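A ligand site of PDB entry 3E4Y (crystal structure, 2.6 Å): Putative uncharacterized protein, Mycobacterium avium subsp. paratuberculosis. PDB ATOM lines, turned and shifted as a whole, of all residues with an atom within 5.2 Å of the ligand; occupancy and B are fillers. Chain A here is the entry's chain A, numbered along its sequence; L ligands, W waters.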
ATOM      1  N   ALA A  17      23.194 -10.602  10.050  1.00  0.00           N
ATOM      2  CA  ALA A  17      21.893 -10.009  10.343  1.00  0.00           C
ATOM      3  C   ALA A  17      22.077  -8.889  11.365  1.00  0.00           C
ATOM      4  O   ALA A  17      21.596  -7.772  11.177  1.00  0.00           O
ATOM      5  CB  ALA A  17      20.928 -11.062  10.885  1.00  0.00           C
ATOM      6  N   ILE A  18      22.799  -9.190  12.444  1.00  0.00           N
ATOM      7  CA  ILE A  18      23.052  -8.191  13.481  1.00  0.00           C
ATOM      8  C   ILE A  18      23.777  -6.988  12.886  1.00  0.00           C
ATOM      9  O   ILE A  18      23.472  -5.833  13.220  1.00  0.00           O
ATOM     10  CB  ILE A  18      23.908  -8.792  14.630  1.00  0.00           C
ATOM     11  CG1 ILE A  18      23.156  -9.928  15.322  1.00  0.00           C
ATOM     12  CG2 ILE A  18      24.202  -7.724  15.671  1.00  0.00           C
ATOM     13  CD1 ILE A  18      21.900  -9.477  16.057  1.00  0.00           C
ATOM     14  N   ILE A  21      21.452  -4.819  11.092  1.00  0.00           N
ATOM     15  CA  ILE A  21      20.647  -4.174  12.124  1.00  0.00           C
ATOM     16  C   ILE A  21      21.400  -2.999  12.751  1.00  0.00           C
ATOM     17  O   ILE A  21      20.858  -1.900  12.876  1.00  0.00           O
ATOM     18  CB  ILE A  21      20.263  -5.172  13.232  1.00  0.00           C
ATOM     19  CG1 ILE A  21      19.274  -6.205  12.681  1.00  0.00           C
ATOM     20  CG2 ILE A  21      19.674  -4.429  14.437  1.00  0.00           C
ATOM     21  CD1 ILE A  21      18.871  -7.248  13.688  1.00  0.00           C
ATOM     22  N   ARG A  32      18.101  -4.910  22.963  1.00  0.00           N
ATOM     23  CA  ARG A  32      17.756  -5.911  21.976  1.00  0.00           C
ATOM     24  C   ARG A  32      18.194  -5.253  20.652  1.00  0.00           C
ATOM     25  O   ARG A  32      17.988  -4.058  20.476  1.00  0.00           O
ATOM     26  CB  ARG A  32      16.245  -6.142  21.980  1.00  0.00           C
ATOM     27  CG  ARG A  32      15.686  -6.613  23.308  1.00  0.00           C
ATOM     28  CD  ARG A  32      14.165  -6.527  23.322  1.00  0.00           C
ATOM     29  NE  ARG A  32      13.566  -7.297  24.406  1.00  0.00           N
ATOM     30  CZ  ARG A  32      13.737  -7.037  25.705  1.00  0.00           C
ATOM     31  NH1 ARG A  32      14.493  -6.017  26.090  1.00  0.00           N
ATOM     32  NH2 ARG A  32      13.174  -7.825  26.606  1.00  0.00           N
ATOM     33  N   ALA A  33      18.805  -6.009  19.746  1.00  0.00           N
ATOM     34  CA  ALA A  33      19.255  -5.425  18.480  1.00  0.00           C
ATOM     35  C   ALA A  33      18.115  -4.617  17.870  1.00  0.00           C
ATOM     36  O   ALA A  33      18.333  -3.519  17.367  1.00  0.00           O
ATOM     37  CB  ALA A  33      19.737  -6.500  17.528  1.00  0.00           C
ATOM     38  N   LEU A  34      16.906  -5.170  17.903  1.00  0.00           N
ATOM     39  CA  LEU A  34      15.723  -4.487  17.400  1.00  0.00           C
ATOM     40  C   LEU A  34      14.699  -4.452  18.530  1.00  0.00           C
ATOM     41  O   LEU A  34      14.825  -5.187  19.502  1.00  0.00           O
ATOM     42  CB  LEU A  34      15.136  -5.211  16.189  1.00  0.00           C
ATOM     43  CG  LEU A  34      16.000  -5.094  14.936  1.00  0.00           C
ATOM     44  CD1 LEU A  34      15.304  -5.807  13.771  1.00  0.00           C
ATOM     45  CD2 LEU A  34      16.225  -3.622  14.597  1.00  0.00           C
ATOM     46  N   HIS A  35      13.685  -3.593  18.408  1.00  0.00           N
ATOM     47  CA  HIS A  35      12.667  -3.484  19.450  1.00  0.00           C
ATOM     48  C   HIS A  35      13.353  -3.185  20.774  1.00  0.00           C
ATOM     49  O   HIS A  35      12.979  -3.719  21.826  1.00  0.00           O
ATOM     50  CB  HIS A  35      11.861  -4.795  19.546  1.00  0.00           C
ATOM     51  CG  HIS A  35      10.952  -5.028  18.370  1.00  0.00           C
ATOM     52  ND1 HIS A  35       9.617  -4.710  18.401  1.00  0.00           N
ATOM     53  CD2 HIS A  35      11.199  -5.509  17.125  1.00  0.00           C
ATOM     54  CE1 HIS A  35       9.073  -4.979  17.217  1.00  0.00           C
ATOM     55  NE2 HIS A  35      10.013  -5.469  16.441  1.00  0.00           N
ATOM     56  N   ARG A  70       5.195  -7.812  26.486  1.00  0.00           N
ATOM     57  CA  ARG A  70       6.111  -6.698  26.248  1.00  0.00           C
ATOM     58  C   ARG A  70       5.601  -5.847  25.076  1.00  0.00           C
ATOM     59  O   ARG A  70       5.346  -6.355  23.979  1.00  0.00           O
ATOM     60  CB  ARG A  70       7.542  -7.173  25.953  1.00  0.00           C
ATOM     61  CG  ARG A  70       8.555  -6.012  25.881  1.00  0.00           C
ATOM     62  CD  ARG A  70       9.995  -6.479  26.096  1.00  0.00           C
ATOM     63  NE  ARG A  70      10.983  -5.397  26.183  1.00  0.00           N
ATOM     64  CZ  ARG A  70      11.446  -4.706  25.150  1.00  0.00           C
ATOM     65  NH1 ARG A  70      11.031  -4.955  23.919  1.00  0.00           N
ATOM     66  NH2 ARG A  70      12.374  -3.773  25.341  1.00  0.00           N
ATOM     67  N   SER A  72       6.486  -2.854  22.597  1.00  0.00           N
ATOM     68  CA  SER A  72       7.704  -2.194  22.145  1.00  0.00           C
ATOM     69  C   SER A  72       7.630  -1.495  20.801  1.00  0.00           C
ATOM     70  O   SER A  72       6.693  -1.689  20.026  1.00  0.00           O
ATOM     71  CB  SER A  72       8.825  -3.222  22.094  1.00  0.00           C
ATOM     72  OG  SER A  72       8.578  -4.170  21.058  1.00  0.00           O
ATOM     73  N   GLY A  89       5.502  -3.547  18.603  1.00  0.00           N
ATOM     74  CA  GLY A  89       5.428  -4.982  18.804  1.00  0.00           C
ATOM     75  C   GLY A  89       4.784  -5.386  20.108  1.00  0.00           C
ATOM     76  O   GLY A  89       4.991  -4.747  21.141  1.00  0.00           O
ATOM     77  N   MET A  90       3.974  -6.438  20.054  1.00  0.00           N
ATOM     78  CA  MET A  90       3.316  -7.004  21.238  1.00  0.00           C
ATOM     79  C   MET A  90       3.745  -8.454  21.355  1.00  0.00           C
ATOM     80  O   MET A  90       3.465  -9.259  20.466  1.00  0.00           O
ATOM     81  CB  MET A  90       1.787  -6.954  21.117  1.00  0.00           C
ATOM     82  CG  MET A  90       1.099  -7.591  22.331  1.00  0.00           C
ATOM     83  SD  MET A  90      -0.697  -7.613  22.293  1.00  0.00           S
ATOM     84  CE  MET A  90      -1.077  -7.839  24.013  1.00  0.00           C
ATOM     85  N   ALA A  91       4.438  -8.783  22.436  1.00  0.00           N
ATOM     86  CA  ALA A  91       4.904 -10.160  22.630  1.00  0.00           C
ATOM     87  C   ALA A  91       4.375 -10.734  23.934  1.00  0.00           C
ATOM     88  O   ALA A  91       4.402 -10.070  24.972  1.00  0.00           O
ATOM     89  CB  ALA A  91       6.432 -10.186  22.612  1.00  0.00           C
ATOM     90  N   SER A 105       4.853 -13.924  19.264  1.00  0.00           N
ATOM     91  CA  SER A 105       5.428 -12.635  18.885  1.00  0.00           C
ATOM     92  C   SER A 105       4.647 -11.963  17.755  1.00  0.00           C
ATOM     93  O   SER A 105       4.400 -12.556  16.701  1.00  0.00           O
ATOM     94  CB  SER A 105       6.873 -12.857  18.439  1.00  0.00           C
ATOM     95  OG  SER A 105       7.491 -11.639  18.085  1.00  0.00           O
ATOM     96  N   ALA A 106       4.237 -10.721  17.983  1.00  0.00           N
ATOM     97  CA  ALA A 106       3.471 -10.019  16.965  1.00  0.00           C
ATOM     98  C   ALA A 106       3.767  -8.532  16.894  1.00  0.00           C
ATOM     99  O   ALA A 106       4.081  -7.915  17.902  1.00  0.00           O
ATOM    100  CB  ALA A 106       1.977 -10.234  17.201  1.00  0.00           C
ATOM    101  N   GLN A 107       3.660  -7.968  15.700  1.00  0.00           N
ATOM    102  CA  GLN A 107       3.886  -6.551  15.510  1.00  0.00           C
ATOM    103  C   GLN A 107       2.786  -5.979  14.629  1.00  0.00           C
ATOM    104  O   GLN A 107       1.980  -6.714  14.063  1.00  0.00           O
ATOM    105  CB  GLN A 107       5.286  -6.307  14.921  1.00  0.00           C
ATOM    106  CG  GLN A 107       5.624  -7.197  13.756  1.00  0.00           C
ATOM    107  CD  GLN A 107       4.795  -6.881  12.559  1.00  0.00           C
ATOM    108  OE1 GLN A 107       4.955  -5.817  11.957  1.00  0.00           O
ATOM    109  NE2 GLN A 107       3.895  -7.794  12.199  1.00  0.00           N
ATOM    110  N   LEU A 112       4.682  -9.721   6.101  1.00  0.00           N
ATOM    111  CA  LEU A 112       6.103  -9.423   6.174  1.00  0.00           C
ATOM    112  C   LEU A 112       6.542  -8.732   4.876  1.00  0.00           C
ATOM    113  O   LEU A 112       6.013  -9.040   3.801  1.00  0.00           O
ATOM    114  CB  LEU A 112       6.904 -10.701   6.412  1.00  0.00           C
ATOM    115  CG  LEU A 112       8.375 -10.534   6.771  1.00  0.00           C
ATOM    116  CD1 LEU A 112       8.543  -9.479   7.853  1.00  0.00           C
ATOM    117  CD2 LEU A 112       8.944 -11.859   7.224  1.00  0.00           C
ATOM    118  N   PRO A 117      14.684 -14.473   4.781  1.00  0.00           N
ATOM    119  CA  PRO A 117      15.545 -13.724   5.693  1.00  0.00           C
ATOM    120  C   PRO A 117      16.494 -12.815   4.883  1.00  0.00           C
ATOM    121  O   PRO A 117      16.706 -11.651   5.238  1.00  0.00           O
ATOM    122  CB  PRO A 117      16.303 -14.818   6.436  1.00  0.00           C
ATOM    123  CG  PRO A 117      15.336 -15.950   6.427  1.00  0.00           C
ATOM    124  CD  PRO A 117      14.816 -15.925   5.013  1.00  0.00           C
ATOM    125  N   PHE A 120      14.815  -9.705   3.791  1.00  0.00           N
ATOM    126  CA  PHE A 120      14.643  -8.772   4.883  1.00  0.00           C
ATOM    127  C   PHE A 120      15.956  -8.079   5.211  1.00  0.00           C
ATOM    128  O   PHE A 120      16.006  -6.858   5.347  1.00  0.00           O
ATOM    129  CB  PHE A 120      14.163  -9.487   6.134  1.00  0.00           C
ATOM    130  CG  PHE A 120      13.737  -8.565   7.225  1.00  0.00           C
ATOM    131  CD1 PHE A 120      12.496  -7.959   7.198  1.00  0.00           C
ATOM    132  CD2 PHE A 120      14.590  -8.288   8.287  1.00  0.00           C
ATOM    133  CE1 PHE A 120      12.100  -7.093   8.208  1.00  0.00           C
ATOM    134  CE2 PHE A 120      14.202  -7.433   9.302  1.00  0.00           C
ATOM    135  CZ  PHE A 120      12.949  -6.830   9.267  1.00  0.00           C
ATOM    136  N   ILE A 121      17.026  -8.856   5.325  1.00  0.00           N
ATOM    137  CA  ILE A 121      18.346  -8.311   5.627  1.00  0.00           C
ATOM    138  C   ILE A 121      18.851  -7.395   4.518  1.00  0.00           C
ATOM    139  O   ILE A 121      19.381  -6.311   4.808  1.00  0.00           O
ATOM    140  CB  ILE A 121      19.383  -9.427   5.855  1.00  0.00           C
ATOM    141  CG1 ILE A 121      18.950 -10.289   7.045  1.00  0.00           C
ATOM    142  CG2 ILE A 121      20.754  -8.806   6.106  1.00  0.00           C
ATOM    143  CD1 ILE A 121      18.721  -9.513   8.333  1.00  0.00           C
ATOM    144  N   HIS A 170       0.091  -8.750  14.571  1.00  0.00           N
ATOM    145  CA  HIS A 170       0.025  -9.979  13.803  1.00  0.00           C
ATOM    146  C   HIS A 170       1.293 -10.825  13.911  1.00  0.00           C
ATOM    147  O   HIS A 170       2.402 -10.298  13.910  1.00  0.00           O
ATOM    148  CB  HIS A 170      -0.259  -9.607  12.340  1.00  0.00           C
ATOM    149  CG  HIS A 170      -1.294  -8.534  12.190  1.00  0.00           C
ATOM    150  ND1 HIS A 170      -2.636  -8.761  12.394  1.00  0.00           N
ATOM    151  CD2 HIS A 170      -1.174  -7.214  11.919  1.00  0.00           C
ATOM    152  CE1 HIS A 170      -3.297  -7.626  12.253  1.00  0.00           C
ATOM    153  NE2 HIS A 170      -2.432  -6.675  11.966  1.00  0.00           N
ATOM    154  N   GLY A 171       1.101 -12.145  14.003  1.00  0.00           N
ATOM    155  CA  GLY A 171       2.233 -13.060  14.108  1.00  0.00           C
ATOM    156  C   GLY A 171       2.896 -13.393  12.778  1.00  0.00           C
ATOM    157  O   GLY A 171       4.014 -13.915  12.756  1.00  0.00           O
ATOM    158  N   LEU A 172       2.202 -13.099  11.684  1.00  0.00           N
ATOM    159  CA  LEU A 172       2.697 -13.322  10.324  1.00  0.00           C
ATOM    160  C   LEU A 172       3.005 -14.767   9.926  1.00  0.00           C
ATOM    161  O   LEU A 172       2.482 -15.246   8.928  1.00  0.00           O
ATOM    162  CB  LEU A 172       3.936 -12.453  10.057  1.00  0.00           C
ATOM    163  CG  LEU A 172       3.754 -10.944  10.293  1.00  0.00           C
ATOM    164  CD1 LEU A 172       5.010 -10.197   9.870  1.00  0.00           C
ATOM    165  CD2 LEU A 172       2.533 -10.443   9.516  1.00  0.00           C
ATOM    166  N   HIS A 173       3.854 -15.457  10.680  1.00  0.00           N
ATOM    167  CA  HIS A 173       4.197 -16.827  10.309  1.00  0.00           C
ATOM    168  C   HIS A 173       3.046 -17.778  10.546  1.00  0.00           C
ATOM    169  O   HIS A 173       2.228 -17.570  11.432  1.00  0.00           O
ATOM    170  CB  HIS A 173       5.408 -17.325  11.086  1.00  0.00           C
ATOM    171  CG  HIS A 173       6.573 -16.394  11.032  1.00  0.00           C
ATOM    172  ND1 HIS A 173       7.168 -16.003   9.847  1.00  0.00           N
ATOM    173  CD2 HIS A 173       7.249 -15.749  12.013  1.00  0.00           C
ATOM    174  CE1 HIS A 173       8.154 -15.166  10.100  1.00  0.00           C
ATOM    175  NE2 HIS A 173       8.225 -14.997  11.413  1.00  0.00           N
ATOM    176  N   VAL A 275      15.010 -11.930  29.306  1.00  0.00           N
ATOM    177  CA  VAL A 275      13.670 -12.117  28.778  1.00  0.00           C
ATOM    178  C   VAL A 275      13.671 -11.975  27.274  1.00  0.00           C
ATOM    179  O   VAL A 275      13.913 -10.893  26.726  1.00  0.00           O
ATOM    180  CB  VAL A 275      12.678 -11.111  29.391  1.00  0.00           C
ATOM    181  CG1 VAL A 275      11.313 -11.252  28.728  1.00  0.00           C
ATOM    182  CG2 VAL A 275      12.536 -11.373  30.889  1.00  0.00           C
ATOM    183  N   VAL A 276      13.423 -13.095  26.590  1.00  0.00           N
ATOM    184  CA  VAL A 276      13.400 -13.112  25.138  1.00  0.00           C
ATOM    185  C   VAL A 276      12.167 -13.847  24.595  1.00  0.00           C
ATOM    186  O   VAL A 276      11.843 -14.940  25.049  1.00  0.00           O
ATOM    187  CB  VAL A 276      14.703 -13.749  24.565  1.00  0.00           C
ATOM    188  CG1 VAL A 276      15.061 -15.003  25.347  1.00  0.00           C
ATOM    189  CG2 VAL A 276      14.536 -14.069  23.084  1.00  0.00           C
ATOM    190  N   PHE A 277      11.467 -13.217  23.658  1.00  0.00           N
ATOM    191  CA  PHE A 277      10.278 -13.828  23.058  1.00  0.00           C
ATOM    192  C   PHE A 277      10.692 -14.397  21.718  1.00  0.00           C
ATOM    193  O   PHE A 277      10.802 -13.672  20.729  1.00  0.00           O
ATOM    194  CB  PHE A 277       9.165 -12.800  22.872  1.00  0.00           C
ATOM    195  CG  PHE A 277       8.726 -12.128  24.136  1.00  0.00           C
ATOM    196  CD1 PHE A 277       9.500 -11.114  24.707  1.00  0.00           C
ATOM    197  CD2 PHE A 277       7.549 -12.509  24.772  1.00  0.00           C
ATOM    198  CE1 PHE A 277       9.094 -10.492  25.897  1.00  0.00           C
ATOM    199  CE2 PHE A 277       7.131 -11.890  25.955  1.00  0.00           C
ATOM    200  CZ  PHE A 277       7.913 -10.884  26.517  1.00  0.00           C
ATOM    201  N   VAL A 293      11.892 -17.448   7.271  1.00  0.00           N
ATOM    202  CA  VAL A 293      12.063 -16.265   8.117  1.00  0.00           C
ATOM    203  C   VAL A 293      11.896 -16.642   9.588  1.00  0.00           C
ATOM    204  O   VAL A 293      12.675 -16.224  10.438  1.00  0.00           O
ATOM    205  CB  VAL A 293      11.037 -15.160   7.757  1.00  0.00           C
ATOM    206  CG1 VAL A 293      11.037 -14.065   8.819  1.00  0.00           C
ATOM    207  CG2 VAL A 293      11.392 -14.562   6.408  1.00  0.00           C
ATOM    208  N   PHE A 296      14.934 -18.580  10.930  1.00  0.00           N
ATOM    209  CA  PHE A 296      16.142 -17.782  11.054  1.00  0.00           C
ATOM    210  C   PHE A 296      16.120 -16.897  12.288  1.00  0.00           C
ATOM    211  O   PHE A 296      17.156 -16.623  12.896  1.00  0.00           O
ATOM    212  CB  PHE A 296      16.320 -16.922   9.808  1.00  0.00           C
ATOM    213  CG  PHE A 296      17.577 -16.112   9.811  1.00  0.00           C
ATOM    214  CD1 PHE A 296      18.812 -16.734   9.814  1.00  0.00           C
ATOM    215  CD2 PHE A 296      17.523 -14.718   9.783  1.00  0.00           C
ATOM    216  CE1 PHE A 296      19.999 -15.979   9.787  1.00  0.00           C
ATOM    217  CE2 PHE A 296      18.692 -13.950   9.751  1.00  0.00           C
ATOM    218  CZ  PHE A 296      19.935 -14.581   9.746  1.00  0.00           C
ATOM    219  N   ARG A 297      14.925 -16.454  12.655  1.00  0.00           N
ATOM    220  CA  ARG A 297      14.765 -15.595  13.806  1.00  0.00           C
ATOM    221  C   ARG A 297      15.407 -16.101  15.095  1.00  0.00           C
ATOM    222  O   ARG A 297      16.204 -15.402  15.712  1.00  0.00           O
ATOM    223  CB  ARG A 297      13.288 -15.337  14.051  1.00  0.00           C
ATOM    224  CG  ARG A 297      12.688 -14.338  13.097  1.00  0.00           C
ATOM    225  CD  ARG A 297      11.756 -13.437  13.864  1.00  0.00           C
ATOM    226  NE  ARG A 297      10.368 -13.820  13.705  1.00  0.00           N
ATOM    227  CZ  ARG A 297       9.423 -13.545  14.603  1.00  0.00           C
ATOM    228  NH1 ARG A 297       9.735 -12.885  15.718  1.00  0.00           N
ATOM    229  NH2 ARG A 297       8.171 -13.914  14.373  1.00  0.00           N
ATOM    230  N   VAL A 300      19.145 -15.431  14.984  1.00  0.00           N
ATOM    231  CA  VAL A 300      19.546 -14.041  15.075  1.00  0.00           C
ATOM    232  C   VAL A 300      19.190 -13.496  16.454  1.00  0.00           C
ATOM    233  O   VAL A 300      19.830 -12.570  16.946  1.00  0.00           O
ATOM    234  CB  VAL A 300      18.890 -13.165  13.972  1.00  0.00           C
ATOM    235  CG1 VAL A 300      17.403 -13.410  13.930  1.00  0.00           C
ATOM    236  CG2 VAL A 300      19.167 -11.699  14.242  1.00  0.00           C
ATOM    237  N   TYR A 301      18.173 -14.076  17.084  1.00  0.00           N
ATOM    238  CA  TYR A 301      17.782 -13.641  18.422  1.00  0.00           C
ATOM    239  C   TYR A 301      18.838 -14.070  19.428  1.00  0.00           C
ATOM    240  O   TYR A 301      19.179 -13.306  20.316  1.00  0.00           O
ATOM    241  CB  TYR A 301      16.431 -14.216  18.840  1.00  0.00           C
ATOM    242  CG  TYR A 301      15.254 -13.552  18.176  1.00  0.00           C
ATOM    243  CD1 TYR A 301      13.981 -13.615  18.745  1.00  0.00           C
ATOM    244  CD2 TYR A 301      15.396 -12.889  16.961  1.00  0.00           C
ATOM    245  CE1 TYR A 301      12.887 -13.035  18.117  1.00  0.00           C
ATOM    246  CE2 TYR A 301      14.307 -12.326  16.330  1.00  0.00           C
ATOM    247  CZ  TYR A 301      13.065 -12.391  16.906  1.00  0.00           C
ATOM    248  OH  TYR A 301      11.999 -11.815  16.248  1.00  0.00           O
ATOM    249  N   SER A 304      21.489 -11.630  19.350  1.00  0.00           N
ATOM    250  CA  SER A 304      21.067 -10.407  20.027  1.00  0.00           C
ATOM    251  C   SER A 304      21.053 -10.561  21.543  1.00  0.00           C
ATOM    252  O   SER A 304      21.515  -9.680  22.272  1.00  0.00           O
ATOM    253  CB  SER A 304      19.668 -10.000  19.557  1.00  0.00           C
ATOM    254  OG  SER A 304      19.236  -8.804  20.193  1.00  0.00           O
ATOM    255  N   VAL A 305      20.516 -11.674  22.016  1.00  0.00           N
ATOM    256  CA  VAL A 305      20.441 -11.944  23.440  1.00  0.00           C
ATOM    257  C   VAL A 305      21.839 -12.025  24.023  1.00  0.00           C
ATOM    258  O   VAL A 305      22.067 -11.652  25.169  1.00  0.00           O
ATOM    259  CB  VAL A 305      19.679 -13.252  23.745  1.00  0.00           C
ATOM    260  CG1 VAL A 305      19.869 -13.652  25.189  1.00  0.00           C
ATOM    261  CG2 VAL A 305      18.206 -13.056  23.462  1.00  0.00           C
ATOM    262  N   ARG A 308      23.505  -8.529  24.596  1.00  0.00           N
ATOM    263  CA  ARG A 308      23.001  -7.767  25.718  1.00  0.00           C
ATOM    264  C   ARG A 308      23.115  -8.471  27.054  1.00  0.00           C
ATOM    265  O   ARG A 308      22.861  -7.871  28.097  1.00  0.00           O
ATOM    266  CB  ARG A 308      21.557  -7.334  25.440  1.00  0.00           C
ATOM    267  CG  ARG A 308      20.569  -8.443  25.112  1.00  0.00           C
ATOM    268  CD  ARG A 308      19.228  -7.851  24.688  1.00  0.00           C
ATOM    269  NE  ARG A 308      18.183  -8.857  24.478  1.00  0.00           N
ATOM    270  CZ  ARG A 308      17.335  -9.278  25.415  1.00  0.00           C
ATOM    271  NH1 ARG A 308      17.397  -8.777  26.640  1.00  0.00           N
ATOM    272  NH2 ARG A 308      16.435 -10.203  25.125  1.00  0.00           N
HETATM  273  C1  LIG L   1      12.499  -8.591  18.395  1.00  0.00           C
HETATM  274  C2  LIG L   1      15.342  -9.574  14.657  1.00  0.00           C
HETATM  275  C3  LIG L   1      11.506 -10.577  11.993  1.00  0.00           C
HETATM  276  C4  LIG L   1       8.642  -9.554  15.709  1.00  0.00           C
HETATM  277  C5  LIG L   1      13.613  -8.809  17.599  1.00  0.00           C
HETATM  278  C6  LIG L   1      14.995  -8.671  18.025  1.00  0.00           C
HETATM  279  C7  LIG L   1      15.777  -8.936  16.965  1.00  0.00           C
HETATM  280  C8  LIG L   1      14.911  -9.253  15.897  1.00  0.00           C
HETATM  281  C9  LIG L   1      17.309  -8.910  16.934  1.00  0.00           C
HETATM  282  C10 LIG L   1      15.527  -8.304  19.405  1.00  0.00           C
HETATM  283  C11 LIG L   1      15.668  -9.736  20.079  1.00  0.00           C
HETATM  284  C12 LIG L   1      16.193  -9.817  21.505  1.00  0.00           C
HETATM  285  O1  LIG L   1      17.208  -9.316  21.829  1.00  0.00           O
HETATM  286  O2  LIG L   1      15.510 -10.485  22.405  1.00  0.00           O
HETATM  287  C13 LIG L   1      14.546  -9.908  13.606  1.00  0.00           C
HETATM  288  C14 LIG L   1      15.086 -10.240  12.321  1.00  0.00           C
HETATM  289  C15 LIG L   1      14.054 -10.535  11.515  1.00  0.00           C
HETATM  290  C16 LIG L   1      12.817 -10.361  12.397  1.00  0.00           C
HETATM  291  C17 LIG L   1      16.574 -10.261  11.938  1.00  0.00           C
HETATM  292  C18 LIG L   1      14.185 -10.948  10.081  1.00  0.00           C
HETATM  293  C19 LIG L   1      14.310 -12.197   9.660  1.00  0.00           C
HETATM  294  C20 LIG L   1      10.374 -10.418  12.771  1.00  0.00           C
HETATM  295  C21 LIG L   1       9.024 -10.654  12.328  1.00  0.00           C
HETATM  296  C22 LIG L   1       8.187 -10.361  13.371  1.00  0.00           C
HETATM  297  C23 LIG L   1       9.062  -9.947  14.471  1.00  0.00           C
HETATM  298  C24 LIG L   1       8.587 -11.124  10.944  1.00  0.00           C
HETATM  299  C25 LIG L   1       6.682 -10.461  13.347  1.00  0.00           C
HETATM  300  C26 LIG L   1       5.959 -11.243  14.149  1.00  0.00           C
HETATM  301  C27 LIG L   1       9.472  -9.179  16.759  1.00  0.00           C
HETATM  302  C28 LIG L   1       8.930  -8.755  18.081  1.00  0.00           C
HETATM  303  C29 LIG L   1       9.964  -8.483  18.840  1.00  0.00           C
HETATM  304  C30 LIG L   1      11.188  -8.738  17.981  1.00  0.00           C
HETATM  305  C31 LIG L   1       7.457  -8.649  18.465  1.00  0.00           C
HETATM  306  C32 LIG L   1       9.846  -7.994  20.294  1.00  0.00           C
HETATM  307  C33 LIG L   1      10.546  -8.854  21.350  1.00  0.00           C
HETATM  308  C34 LIG L   1      10.374  -8.256  22.743  1.00  0.00           C
HETATM  309  O3  LIG L   1       9.762  -7.232  22.949  1.00  0.00           O
HETATM  310  O4  LIG L   1      10.945  -8.874  23.755  1.00  0.00           O
HETATM  311  N1  LIG L   1      13.558  -9.198  16.271  1.00  0.00           N
HETATM  312  N2  LIG L   1      13.190  -9.975  13.644  1.00  0.00           N
HETATM  313  N3  LIG L   1      10.392 -10.008  14.081  1.00  0.00           N
HETATM  314  N4  LIG L   1      10.810  -9.140  16.745  1.00  0.00           N
HETATM  315 FE1  LIG L   1      11.960  -9.584  15.179  1.00  0.00          FE
HETATM  316  O   HOH W   1       5.687 -14.571  15.176  1.00  0.00           O
HETATM  317  O   HOH W   2       9.841 -11.787  19.232  1.00  0.00           O
HETATM  318  O   HOH W   3      12.690 -10.828  22.811  1.00  0.00           O
HETATM  319  O   HOH W   4       7.375  -6.383  21.892  1.00  0.00           O
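The guanidinium group (NH1) of Arg 70 is in hydrogen-bond range of the backbone carbonyl oxygen (O) of His 35.
NH2 of Arg 308 is in hydrogen-bond range of O of Val 275 (3.1 Å).
The side-chain hydroxyl of Ser 105 lies within hydrogen-bond range of the guanidinium group of Arg 297 (3.5 Å).
The guanidinium group of Arg 32 sits at hydrogen-bond distance from the backbone carbonyl oxygen of Val 275.
A ring nitrogen (NE2) of His 173 lies close to the guanidinium group of Arg 297.
OG of Ser 72 sits at hydrogen-bond distance from ND1 of His 35 (2.9 Å).
O of Ala 106 is in hydrogen-bond range of N of Met 90 (2.6 Å).
O of Ser 72 lies within hydrogen-bond range of N of Gly 89 (2.6 Å).
Water W4 lies within hydrogen-bond range of the side-chain hydroxyl (OG) of Ser 72 (2.7 Å), an oxygen (O3) of the ligand (2.7 Å), the backbone carbonyl oxygen (O) of Arg 70 (2.9 Å) and the backbone carbonyl oxygen (O) of Gly 89 (3.0 Å).
Water W3 bridges an oxygen (O4) of the ligand (2.8 Å) and the backbone NH of Phe 277 (2.8 Å).
Water W2 bridges O of Phe 277 (2.6 Å) and OG of Ser 105 (2.6 Å).
Water W1 lies within hydrogen-bond range of NH2 of Arg 297, O of Ser 105 and O of Gly 171.
The side-chain hydroxyl (OH) of Tyr 301 binds an iron atom (FE1) of the ligand (2.5 Å).
An oxygen (O1) of the ligand sits at hydrogen-bond distance from the side-chain hydroxyl (OG) of Ser 304, 2.7 Å away.
The guanidinium group (NH1) of Arg 70 lies within salt-bridge range of an oxygen (O3) of the ligand (2.8 Å).
NE of Arg 308 lies within salt-bridge range of O1 of the ligand (2.9 Å).
The guanidinium group (NE) of Arg 32 is in salt-bridge range of an oxygen (O4) of the ligand, 3.1 Å away.
A nitrogen (N3) of the ligand lies close to the guanidinium group of Arg 297 (3.4 Å).
CD1 of Ile 21 touches C9 of the ligand (3.97 Å).
CB of Ala 33 touches C9 of the ligand, 3.5 Å away.
Leu 34 touches the ligand (O to C10, 3.2 Å).
CD2 of His 35 touches C30 of the ligand, at 3.3 Å.
Ser 72 touches the ligand (OG to O3, 3.8 Å).
Ser 105 touches the ligand (OG to C31, 3.0 Å).
Ala 106 touches the ligand (O to C31, 3.5 Å).
Gln 107 touches the ligand (CG to C25, 3.5 Å).
CD1 of Leu 112 touches C24 of the ligand (3.5 Å).
Phe 120 touches the ligand (CD2 to C18, 3.2 Å).
His 170 touches the ligand.
O of Gly 171 touches C26 of the ligand, 3.6 Å away.
CD1 of Leu 172 touches C24 of the ligand, at 3.8 Å.
His 173 touches the ligand (NE2 to C24, 3.9 Å).
Val 276 touches the ligand (CG2 to O2, 3.8 Å).
Phe 277 touches the ligand.
Val 293 touches the ligand.
Val 300 touches the ligand.
CG2 of Val 305 touches O2 of the ligand, at 3.9 Å.
Hydrophobic or aromatic side chains that line the ligand: Ile 21, Ala 33, Leu 34, His 35, Leu 112, Phe 120, Leu 172, Val 276, Phe 277, Val 293, Val 300, Tyr 301 and Val 305.
Of the 34 residues printed, 25 come within 4 Å of the ligand.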
